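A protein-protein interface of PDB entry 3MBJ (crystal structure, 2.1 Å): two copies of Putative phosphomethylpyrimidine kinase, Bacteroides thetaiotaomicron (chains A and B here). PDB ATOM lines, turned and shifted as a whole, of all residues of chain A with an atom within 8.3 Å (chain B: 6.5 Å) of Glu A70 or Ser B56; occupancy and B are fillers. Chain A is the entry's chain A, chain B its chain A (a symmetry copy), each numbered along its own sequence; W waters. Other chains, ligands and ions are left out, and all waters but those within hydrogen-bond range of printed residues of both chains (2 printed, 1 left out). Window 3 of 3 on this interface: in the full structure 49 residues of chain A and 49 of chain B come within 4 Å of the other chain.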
ATOM      1  N   LEU A  41     -30.136 -25.734  -4.854  1.00  0.00           N
ATOM      2  CA  LEU A  41     -29.234 -24.645  -5.159  1.00  0.00           C
ATOM      3  C   LEU A  41     -30.012 -23.355  -4.825  1.00  0.00           C
ATOM      4  O   LEU A  41     -30.696 -22.774  -5.675  1.00  0.00           O
ATOM      5  CB  LEU A  41     -28.829 -24.665  -6.646  1.00  0.00           C
ATOM      6  CG  LEU A  41     -27.795 -23.611  -7.154  1.00  0.00           C
ATOM      7  CD1 LEU A  41     -26.479 -23.636  -6.384  1.00  0.00           C
ATOM      8  CD2 LEU A  41     -27.521 -23.809  -8.658  1.00  0.00           C
ATOM      9  N   GLU A  63     -23.081 -17.039  -3.524  1.00  0.00           N
ATOM     10  CA  GLU A  63     -22.799 -18.410  -3.070  1.00  0.00           C
ATOM     11  C   GLU A  63     -23.121 -19.455  -4.162  1.00  0.00           C
ATOM     12  O   GLU A  63     -22.497 -20.511  -4.207  1.00  0.00           O
ATOM     13  CB  GLU A  63     -23.546 -18.727  -1.767  1.00  0.00           C
ATOM     14  CG  GLU A  63     -23.012 -19.969  -1.037  1.00  0.00           C
ATOM     15  CD  GLU A  63     -21.609 -19.798  -0.470  1.00  0.00           C
ATOM     16  OE1 GLU A  63     -21.103 -18.655  -0.451  1.00  0.00           O
ATOM     17  OE2 GLU A  63     -21.016 -20.819  -0.026  1.00  0.00           O
ATOM     18  N   MET A  64     -24.071 -19.161  -5.043  1.00  0.00           N
ATOM     19  CA  MET A  64     -24.486 -20.138  -6.057  1.00  0.00           C
ATOM     20  C   MET A  64     -23.313 -20.773  -6.804  1.00  0.00           C
ATOM     21  O   MET A  64     -23.238 -22.014  -6.867  1.00  0.00           O
ATOM     22  CB  MET A  64     -25.529 -19.557  -7.021  1.00  0.00           C
ATOM     23  CG  MET A  64     -26.867 -19.376  -6.361  1.00  0.00           C
ATOM     24  SD  MET A  64     -28.134 -18.308  -7.375  1.00  0.00           S
ATOM     25  CE  MET A  64     -28.712 -19.717  -8.499  1.00  0.00           C
ATOM     26  N   PRO A  65     -22.381 -19.955  -7.350  1.00  0.00           N
ATOM     27  CA  PRO A  65     -21.249 -20.528  -8.102  1.00  0.00           C
ATOM     28  C   PRO A  65     -20.299 -21.381  -7.277  1.00  0.00           C
ATOM     29  O   PRO A  65     -19.704 -22.321  -7.809  1.00  0.00           O
ATOM     30  CB  PRO A  65     -20.507 -19.294  -8.645  1.00  0.00           C
ATOM     31  CG  PRO A  65     -21.555 -18.190  -8.657  1.00  0.00           C
ATOM     32  CD  PRO A  65     -22.399 -18.483  -7.440  1.00  0.00           C
ATOM     33  N   LYS A  66     -20.158 -21.052  -5.999  1.00  0.00           N
ATOM     34  CA  LYS A  66     -19.337 -21.820  -5.076  1.00  0.00           C
ATOM     35  C   LYS A  66     -19.906 -23.228  -4.830  1.00  0.00           C
ATOM     36  O   LYS A  66     -19.158 -24.202  -4.775  1.00  0.00           O
ATOM     37  CB  LYS A  66     -19.197 -21.050  -3.752  1.00  0.00           C
ATOM     38  CG  LYS A  66     -18.424 -19.717  -3.899  1.00  0.00           C
ATOM     39  CD  LYS A  66     -18.583 -18.809  -2.676  1.00  0.00           C
ATOM     40  CE  LYS A  66     -17.686 -17.579  -2.749  1.00  0.00           C
ATOM     41  NZ  LYS A  66     -17.639 -16.922  -1.392  1.00  0.00           N
ATOM     42  N   ILE A  67     -21.217 -23.312  -4.674  1.00  0.00           N
ATOM     43  CA  ILE A  67     -21.920 -24.597  -4.532  1.00  0.00           C
ATOM     44  C   ILE A  67     -21.734 -25.444  -5.779  1.00  0.00           C
ATOM     45  O   ILE A  67     -21.382 -26.615  -5.694  1.00  0.00           O
ATOM     46  CB  ILE A  67     -23.452 -24.376  -4.247  1.00  0.00           C
ATOM     47  CG1 ILE A  67     -23.652 -23.808  -2.811  1.00  0.00           C
ATOM     48  CG2 ILE A  67     -24.259 -25.703  -4.464  1.00  0.00           C
ATOM     49  CD1 ILE A  67     -24.985 -23.144  -2.580  1.00  0.00           C
ATOM     50  N   ILE A  68     -21.931 -24.820  -6.939  1.00  0.00           N
ATOM     51  CA  ILE A  68     -21.783 -25.468  -8.228  1.00  0.00           C
ATOM     52  C   ILE A  68     -20.362 -25.957  -8.450  1.00  0.00           C
ATOM     53  O   ILE A  68     -20.177 -27.050  -8.990  1.00  0.00           O
ATOM     54  CB  ILE A  68     -22.199 -24.519  -9.396  1.00  0.00           C
ATOM     55  CG1 ILE A  68     -23.695 -24.187  -9.268  1.00  0.00           C
ATOM     56  CG2 ILE A  68     -21.787 -25.113 -10.784  1.00  0.00           C
ATOM     57  CD1 ILE A  68     -24.225 -22.996 -10.202  1.00  0.00           C
ATOM     58  N   ALA A  69     -19.368 -25.171  -8.054  1.00  0.00           N
ATOM     59  CA  ALA A  69     -17.982 -25.595  -8.189  1.00  0.00           C
ATOM     60  C   ALA A  69     -17.749 -26.886  -7.388  1.00  0.00           C
ATOM     61  O   ALA A  69     -17.049 -27.789  -7.843  1.00  0.00           O
ATOM     62  CB  ALA A  69     -16.952 -24.454  -7.755  1.00  0.00           C
ATOM     63  N   GLU A  70     -18.345 -26.980  -6.207  1.00  0.00           N
ATOM     64  CA  GLU A  70     -18.242 -28.189  -5.407  1.00  0.00           C
ATOM     65  C   GLU A  70     -18.978 -29.384  -6.035  1.00  0.00           C
ATOM     66  O   GLU A  70     -18.445 -30.500  -6.038  1.00  0.00           O
ATOM     67  CB  GLU A  70     -18.743 -27.921  -3.990  1.00  0.00           C
ATOM     68  CG  GLU A  70     -17.878 -26.934  -3.220  1.00  0.00           C
ATOM     69  CD  GLU A  70     -16.409 -27.318  -3.159  1.00  0.00           C
ATOM     70  OE1 GLU A  70     -16.082 -28.520  -3.098  1.00  0.00           O
ATOM     71  OE2 GLU A  70     -15.549 -26.415  -3.199  1.00  0.00           O
ATOM     72  N   TRP A  71     -20.178 -29.159  -6.571  1.00  0.00           N
ATOM     73  CA  TRP A  71     -20.914 -30.201  -7.251  1.00  0.00           C
ATOM     74  C   TRP A  71     -20.158 -30.779  -8.424  1.00  0.00           C
ATOM     75  O   TRP A  71     -20.273 -31.982  -8.699  1.00  0.00           O
ATOM     76  CB  TRP A  71     -22.301 -29.712  -7.730  1.00  0.00           C
ATOM     77  CG  TRP A  71     -23.315 -29.502  -6.618  1.00  0.00           C
ATOM     78  CD1 TRP A  71     -23.147 -29.782  -5.282  1.00  0.00           C
ATOM     79  CD2 TRP A  71     -24.610 -28.943  -6.738  1.00  0.00           C
ATOM     80  NE1 TRP A  71     -24.259 -29.445  -4.583  1.00  0.00           N
ATOM     81  CE2 TRP A  71     -25.188 -28.949  -5.446  1.00  0.00           C
ATOM     82  CE3 TRP A  71     -25.351 -28.452  -7.802  1.00  0.00           C
ATOM     83  CZ2 TRP A  71     -26.460 -28.472  -5.195  1.00  0.00           C
ATOM     84  CZ3 TRP A  71     -26.625 -28.006  -7.561  1.00  0.00           C
ATOM     85  CH2 TRP A  71     -27.168 -28.010  -6.258  1.00  0.00           C
ATOM     86  N   LYS A  72     -19.402 -29.936  -9.127  1.00  0.00           N
ATOM     87  CA  LYS A  72     -18.517 -30.393 -10.228  1.00  0.00           C
ATOM     88  C   LYS A  72     -17.440 -31.317  -9.704  1.00  0.00           C
ATOM     89  O   LYS A  72     -17.150 -32.356 -10.301  1.00  0.00           O
ATOM     90  CB  LYS A  72     -17.830 -29.215 -10.928  1.00  0.00           C
ATOM     91  CG  LYS A  72     -18.741 -28.432 -11.885  1.00  0.00           C
ATOM     92  CD  LYS A  72     -17.935 -27.450 -12.787  1.00  0.00           C
ATOM     93  CE  LYS A  72     -18.880 -26.556 -13.611  1.00  0.00           C
ATOM     94  NZ  LYS A  72     -18.161 -25.638 -14.541  1.00  0.00           N
ATOM     95  N   LYS A  73     -16.868 -30.957  -8.566  1.00  0.00           N
ATOM     96  CA  LYS A  73     -15.818 -31.774  -7.948  1.00  0.00           C
ATOM     97  C   LYS A  73     -16.377 -33.121  -7.486  1.00  0.00           C
ATOM     98  O   LYS A  73     -15.714 -34.125  -7.609  1.00  0.00           O
ATOM     99  CB  LYS A  73     -15.184 -31.044  -6.774  1.00  0.00           C
ATOM    100  CG  LYS A  73     -14.407 -29.806  -7.173  1.00  0.00           C
ATOM    101  CD  LYS A  73     -13.889 -29.008  -5.949  1.00  0.00           C
ATOM    102  CE  LYS A  73     -13.372 -27.638  -6.406  1.00  0.00           C
ATOM    103  NZ  LYS A  73     -12.552 -26.905  -5.364  1.00  0.00           N
ATOM    104  N   LEU A  74     -17.602 -33.124  -6.963  1.00  0.00           N
ATOM    105  CA  LEU A  74     -18.294 -34.369  -6.591  1.00  0.00           C
ATOM    106  C   LEU A  74     -18.752 -35.202  -7.810  1.00  0.00           C
ATOM    107  O   LEU A  74     -19.119 -36.348  -7.660  1.00  0.00           O
ATOM    108  CB  LEU A  74     -19.520 -34.083  -5.715  1.00  0.00           C
ATOM    109  CG  LEU A  74     -19.388 -33.394  -4.356  1.00  0.00           C
ATOM    110  CD1 LEU A  74     -20.821 -33.239  -3.765  1.00  0.00           C
ATOM    111  CD2 LEU A  74     -18.472 -34.166  -3.430  1.00  0.00           C
ATOM    112  N   GLU A  75     -18.713 -34.620  -9.007  1.00  0.00           N
ATOM    113  CA  GLU A  75     -19.198 -35.267 -10.233  1.00  0.00           C
ATOM    114  C   GLU A  75     -20.631 -35.760 -10.134  1.00  0.00           C
ATOM    115  O   GLU A  75     -20.971 -36.801 -10.673  1.00  0.00           O
ATOM    116  CB  GLU A  75     -18.254 -36.377 -10.665  1.00  0.00           C
ATOM    117  CG  GLU A  75     -16.916 -35.795 -11.109  1.00  0.00           C
ATOM    118  CD  GLU A  75     -15.844 -36.823 -11.431  1.00  0.00           C
ATOM    119  OE1 GLU A  75     -16.140 -37.888 -11.999  1.00  0.00           O
ATOM    120  OE2 GLU A  75     -14.669 -36.532 -11.141  1.00  0.00           O
ATOM    121  N   VAL A  76     -21.480 -34.986  -9.461  1.00  0.00           N
ATOM    122  CA  VAL A  76     -22.887 -35.342  -9.318  1.00  0.00           C
ATOM    123  C   VAL A  76     -23.555 -35.277 -10.696  1.00  0.00           C
ATOM    124  O   VAL A  76     -23.295 -34.378 -11.462  1.00  0.00           O
ATOM    125  CB  VAL A  76     -23.640 -34.496  -8.221  1.00  0.00           C
ATOM    126  CG1 VAL A  76     -23.312 -33.031  -8.274  1.00  0.00           C
ATOM    127  CG2 VAL A  76     -25.149 -34.724  -8.300  1.00  0.00           C
ATOM    128  N   PHE A 102     -23.998 -29.150 -16.679  1.00  0.00           N
ATOM    129  CA  PHE A 102     -24.481 -30.375 -15.996  1.00  0.00           C
ATOM    130  C   PHE A 102     -25.499 -31.180 -16.814  1.00  0.00           C
ATOM    131  O   PHE A 102     -25.885 -32.275 -16.392  1.00  0.00           O
ATOM    132  CB  PHE A 102     -25.065 -30.038 -14.619  1.00  0.00           C
ATOM    133  CG  PHE A 102     -24.016 -29.831 -13.548  1.00  0.00           C
ATOM    134  CD1 PHE A 102     -23.295 -28.639 -13.476  1.00  0.00           C
ATOM    135  CD2 PHE A 102     -23.735 -30.830 -12.634  1.00  0.00           C
ATOM    136  CE1 PHE A 102     -22.338 -28.442 -12.512  1.00  0.00           C
ATOM    137  CE2 PHE A 102     -22.777 -30.627 -11.645  1.00  0.00           C
ATOM    138  CZ  PHE A 102     -22.069 -29.440 -11.594  1.00  0.00           C
ATOM    139  N   VAL B  45     -25.496 -22.501   4.781  1.00  0.00           N
ATOM    140  CA  VAL B  45     -25.733 -23.128   3.465  1.00  0.00           C
ATOM    141  C   VAL B  45     -24.451 -23.802   3.025  1.00  0.00           C
ATOM    142  O   VAL B  45     -23.388 -23.170   3.013  1.00  0.00           O
ATOM    143  CB  VAL B  45     -26.170 -22.110   2.403  1.00  0.00           C
ATOM    144  CG1 VAL B  45     -26.238 -22.772   1.039  1.00  0.00           C
ATOM    145  CG2 VAL B  45     -27.498 -21.464   2.799  1.00  0.00           C
ATOM    146  N   LEU B  46     -24.549 -25.077   2.663  1.00  0.00           N
ATOM    147  CA  LEU B  46     -23.410 -25.895   2.248  1.00  0.00           C
ATOM    148  C   LEU B  46     -23.699 -26.577   0.919  1.00  0.00           C
ATOM    149  O   LEU B  46     -24.839 -26.946   0.644  1.00  0.00           O
ATOM    150  CB  LEU B  46     -23.129 -26.967   3.303  1.00  0.00           C
ATOM    151  CG  LEU B  46     -22.595 -26.529   4.678  1.00  0.00           C
ATOM    152  CD1 LEU B  46     -23.705 -26.235   5.678  1.00  0.00           C
ATOM    153  CD2 LEU B  46     -21.659 -27.581   5.229  1.00  0.00           C
ATOM    154  N   SER B  47     -22.677 -26.767   0.094  1.00  0.00           N
ATOM    155  CA  SER B  47     -22.837 -27.544  -1.118  1.00  0.00           C
ATOM    156  C   SER B  47     -23.139 -28.988  -0.769  1.00  0.00           C
ATOM    157  O   SER B  47     -23.809 -29.684  -1.519  1.00  0.00           O
ATOM    158  CB  SER B  47     -21.555 -27.516  -1.921  1.00  0.00           C
ATOM    159  OG  SER B  47     -20.486 -28.074  -1.173  1.00  0.00           O
ATOM    160  N   ASN B  48     -22.592 -29.439   0.357  1.00  0.00           N
ATOM    161  CA  ASN B  48     -22.660 -30.839   0.760  1.00  0.00           C
ATOM    162  C   ASN B  48     -22.120 -31.005   2.162  1.00  0.00           C
ATOM    163  O   ASN B  48     -21.403 -30.158   2.656  1.00  0.00           O
ATOM    164  CB  ASN B  48     -21.878 -31.735  -0.213  1.00  0.00           C
ATOM    165  CG  ASN B  48     -20.477 -31.244  -0.463  1.00  0.00           C
ATOM    166  OD1 ASN B  48     -20.227 -30.537  -1.443  1.00  0.00           O
ATOM    167  ND2 ASN B  48     -19.554 -31.594   0.426  1.00  0.00           N
ATOM    168  N   PRO B  53     -14.674 -34.689   0.887  1.00  0.00           N
ATOM    169  CA  PRO B  53     -13.375 -34.046   1.133  1.00  0.00           C
ATOM    170  C   PRO B  53     -13.450 -32.520   1.189  1.00  0.00           C
ATOM    171  O   PRO B  53     -12.859 -31.923   2.063  1.00  0.00           O
ATOM    172  CB  PRO B  53     -12.502 -34.500  -0.036  1.00  0.00           C
ATOM    173  CG  PRO B  53     -13.428 -35.106  -1.058  1.00  0.00           C
ATOM    174  CD  PRO B  53     -14.691 -35.508  -0.336  1.00  0.00           C
ATOM    175  N   GLY B  54     -14.180 -31.898   0.269  1.00  0.00           N
ATOM    176  CA  GLY B  54     -14.399 -30.439   0.303  1.00  0.00           C
ATOM    177  C   GLY B  54     -15.886 -30.120   0.378  1.00  0.00           C
ATOM    178  O   GLY B  54     -16.739 -31.011   0.170  1.00  0.00           O
ATOM    179  N   PHE B  55     -16.192 -28.859   0.672  1.00  0.00           N
ATOM    180  CA  PHE B  55     -17.565 -28.350   0.706  1.00  0.00           C
ATOM    181  C   PHE B  55     -17.552 -26.838   0.685  1.00  0.00           C
ATOM    182  O   PHE B  55     -16.649 -26.224   1.244  1.00  0.00           O
ATOM    183  CB  PHE B  55     -18.272 -28.797   1.989  1.00  0.00           C
ATOM    184  CG  PHE B  55     -17.525 -28.431   3.266  1.00  0.00           C
ATOM    185  CD1 PHE B  55     -16.449 -29.202   3.704  1.00  0.00           C
ATOM    186  CD2 PHE B  55     -17.896 -27.313   4.016  1.00  0.00           C
ATOM    187  CE1 PHE B  55     -15.749 -28.870   4.869  1.00  0.00           C
ATOM    188  CE2 PHE B  55     -17.212 -26.991   5.163  1.00  0.00           C
ATOM    189  CZ  PHE B  55     -16.114 -27.780   5.584  1.00  0.00           C
ATOM    190  N   SER B  56     -18.557 -26.226   0.078  1.00  0.00           N
ATOM    191  CA  SER B  56     -18.741 -24.814   0.271  1.00  0.00           C
ATOM    192  C   SER B  56     -19.430 -24.638   1.618  1.00  0.00           C
ATOM    193  O   SER B  56     -20.132 -25.538   2.109  1.00  0.00           O
ATOM    194  CB  SER B  56     -19.561 -24.198  -0.849  1.00  0.00           C
ATOM    195  OG  SER B  56     -20.893 -24.622  -0.803  1.00  0.00           O
ATOM    196  N   PHE B  57     -19.214 -23.475   2.226  1.00  0.00           N
ATOM    197  CA  PHE B  57     -19.850 -23.178   3.494  1.00  0.00           C
ATOM    198  C   PHE B  57     -20.130 -21.702   3.634  1.00  0.00           C
ATOM    199  O   PHE B  57     -19.216 -20.890   3.545  1.00  0.00           O
ATOM    200  CB  PHE B  57     -18.974 -23.671   4.658  1.00  0.00           C
ATOM    201  CG  PHE B  57     -19.500 -23.286   6.006  1.00  0.00           C
ATOM    202  CD1 PHE B  57     -20.486 -24.039   6.615  1.00  0.00           C
ATOM    203  CD2 PHE B  57     -19.009 -22.161   6.658  1.00  0.00           C
ATOM    204  CE1 PHE B  57     -20.980 -23.684   7.875  1.00  0.00           C
ATOM    205  CE2 PHE B  57     -19.489 -21.810   7.886  1.00  0.00           C
ATOM    206  CZ  PHE B  57     -20.490 -22.588   8.497  1.00  0.00           C
ATOM    207  N   LEU B  58     -21.400 -21.362   3.883  1.00  0.00           N
ATOM    208  CA  LEU B  58     -21.815 -19.984   4.139  1.00  0.00           C
ATOM    209  C   LEU B  58     -22.529 -19.937   5.474  1.00  0.00           C
ATOM    210  O   LEU B  58     -23.634 -20.477   5.603  1.00  0.00           O
ATOM    211  CB  LEU B  58     -22.727 -19.441   3.034  1.00  0.00           C
ATOM    212  CG  LEU B  58     -23.171 -17.981   3.251  1.00  0.00           C
ATOM    213  CD1 LEU B  58     -21.980 -16.989   3.070  1.00  0.00           C
ATOM    214  CD2 LEU B  58     -24.320 -17.644   2.345  1.00  0.00           C
HETATM  215  O   HOH W   1     -22.361 -22.872   0.428  1.00  0.00           O
HETATM  216  O   HOH W   2     -18.642 -21.005   0.295  1.00  0.00           O
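Of the 10 printed residues of chain B, 8 touch a printed residue of chain A.
Printed residues of chain B that touch a printed residue of chain A: Val B45, Ser B47, Asn B48, Gly B54, Phe B55, Ser B56, Phe B57 and Leu B58.
Hydrophobic or aromatic side chains of chain B within 4 Å of the printed part of chain A: Val B45 and Leu B58.
Among the printed residues, 14 pairs touch across the chains.
Among the printed residues, no Asp or Glu carboxylate lies within 4 Å of a Lys or Arg side-chain nitrogen of the other chain.
Leu B58 touches Glu A63 (CB to CD, 3.7 Å).
Ser B56 touches Lys A66.
CG1 of Val B45 touches CD1 of Ile A67, 3.8 Å away.
O of Ile A67 touches CB of Ser B47, 3.9 Å away.
CG1 of Ile A67 touches OG of Ser B56, at 3.5 Å.
Asn B48 touches Glu A70.
C of Gly B54 touches OE1 of Glu A70, at 3.8 Å.
OE1 of Glu A70 touches N of Phe B55, 3.8 Å away.
N of Ser B56 touches CG of Glu A70 (3.4 Å).
CD1 of Leu A74 touches OD1 of Asn B48 (3.6 Å).
NE1 of Trp A71 is in hydrogen-bond range of O of Ser B47 (3.1 Å).
Leu A41 touches none of the printed residues of chain B.
Pro A65 touches none of the printed residues of chain B.
Of chain B, only Ser B47 (3.3 Å), Asn B48 (3.9 Å), Gly B54 (3.8 Å), Phe B55 (3.8 Å) and Ser B56 (3.4 Å) come within 4 Å of Glu A70.
Of the printed residues of chain A, Val B45 touches Ile A67 (3.8 Å).
Of the printed residues of chain A, Ser B47 touches Ile A67, Glu A70 and Trp A71.
Of the printed residues of chain A, Asn B48 touches Glu A70 (3.9 Å) and Leu A74 (3.6 Å).
Of the printed residues of chain A, Phe B55 touches Glu A70 (3.8 Å).
Ser B56 touches just these residues of chain A: Glu A63 (3.8 Å), Lys A66 (3.9 Å), Ile A67 (3.5 Å) and Glu A70 (3.4 Å).
The nearest printed residue of chain A that does not touch Phe B57 is Lys A66 (6.5 Å).
No position is printed for both chains.
The backbone carbonyl oxygen of Val B45 sits at hydrogen-bond distance from the backbone NH of Leu B58 (2.8 Å).
The backbone carbonyl oxygen of Trp A71 lies close to the backbone NH of Val A76, 3.3 Å away.
OG of Ser B56 sits at hydrogen-bond distance from N of Ser B47.
The side-chain carboxylate (OE1) of Glu A63 lies within salt-bridge range of the side-chain amino group (NZ) of Lys A66.
OE2 of Glu A70 lies within salt-bridge range of NZ of Lys A73 (3.7 Å).
The side-chain amide nitrogen of Asn B48 lies within hydrogen-bond range of the backbone carbonyl oxygen of Gly B54, at 2.9 Å.
Water W2 bridges OE2 of Glu A63 (2.4 Å) and N of Phe B57 (3.2 Å).
Water W1 lies within hydrogen-bond range of the side-chain carboxylate (OE2) of Glu A63 (2.5 Å), the side-chain hydroxyl (OG) of Ser B56 (2.6 Å) and the backbone carbonyl oxygen (O) of Val B45 (2.8 Å).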
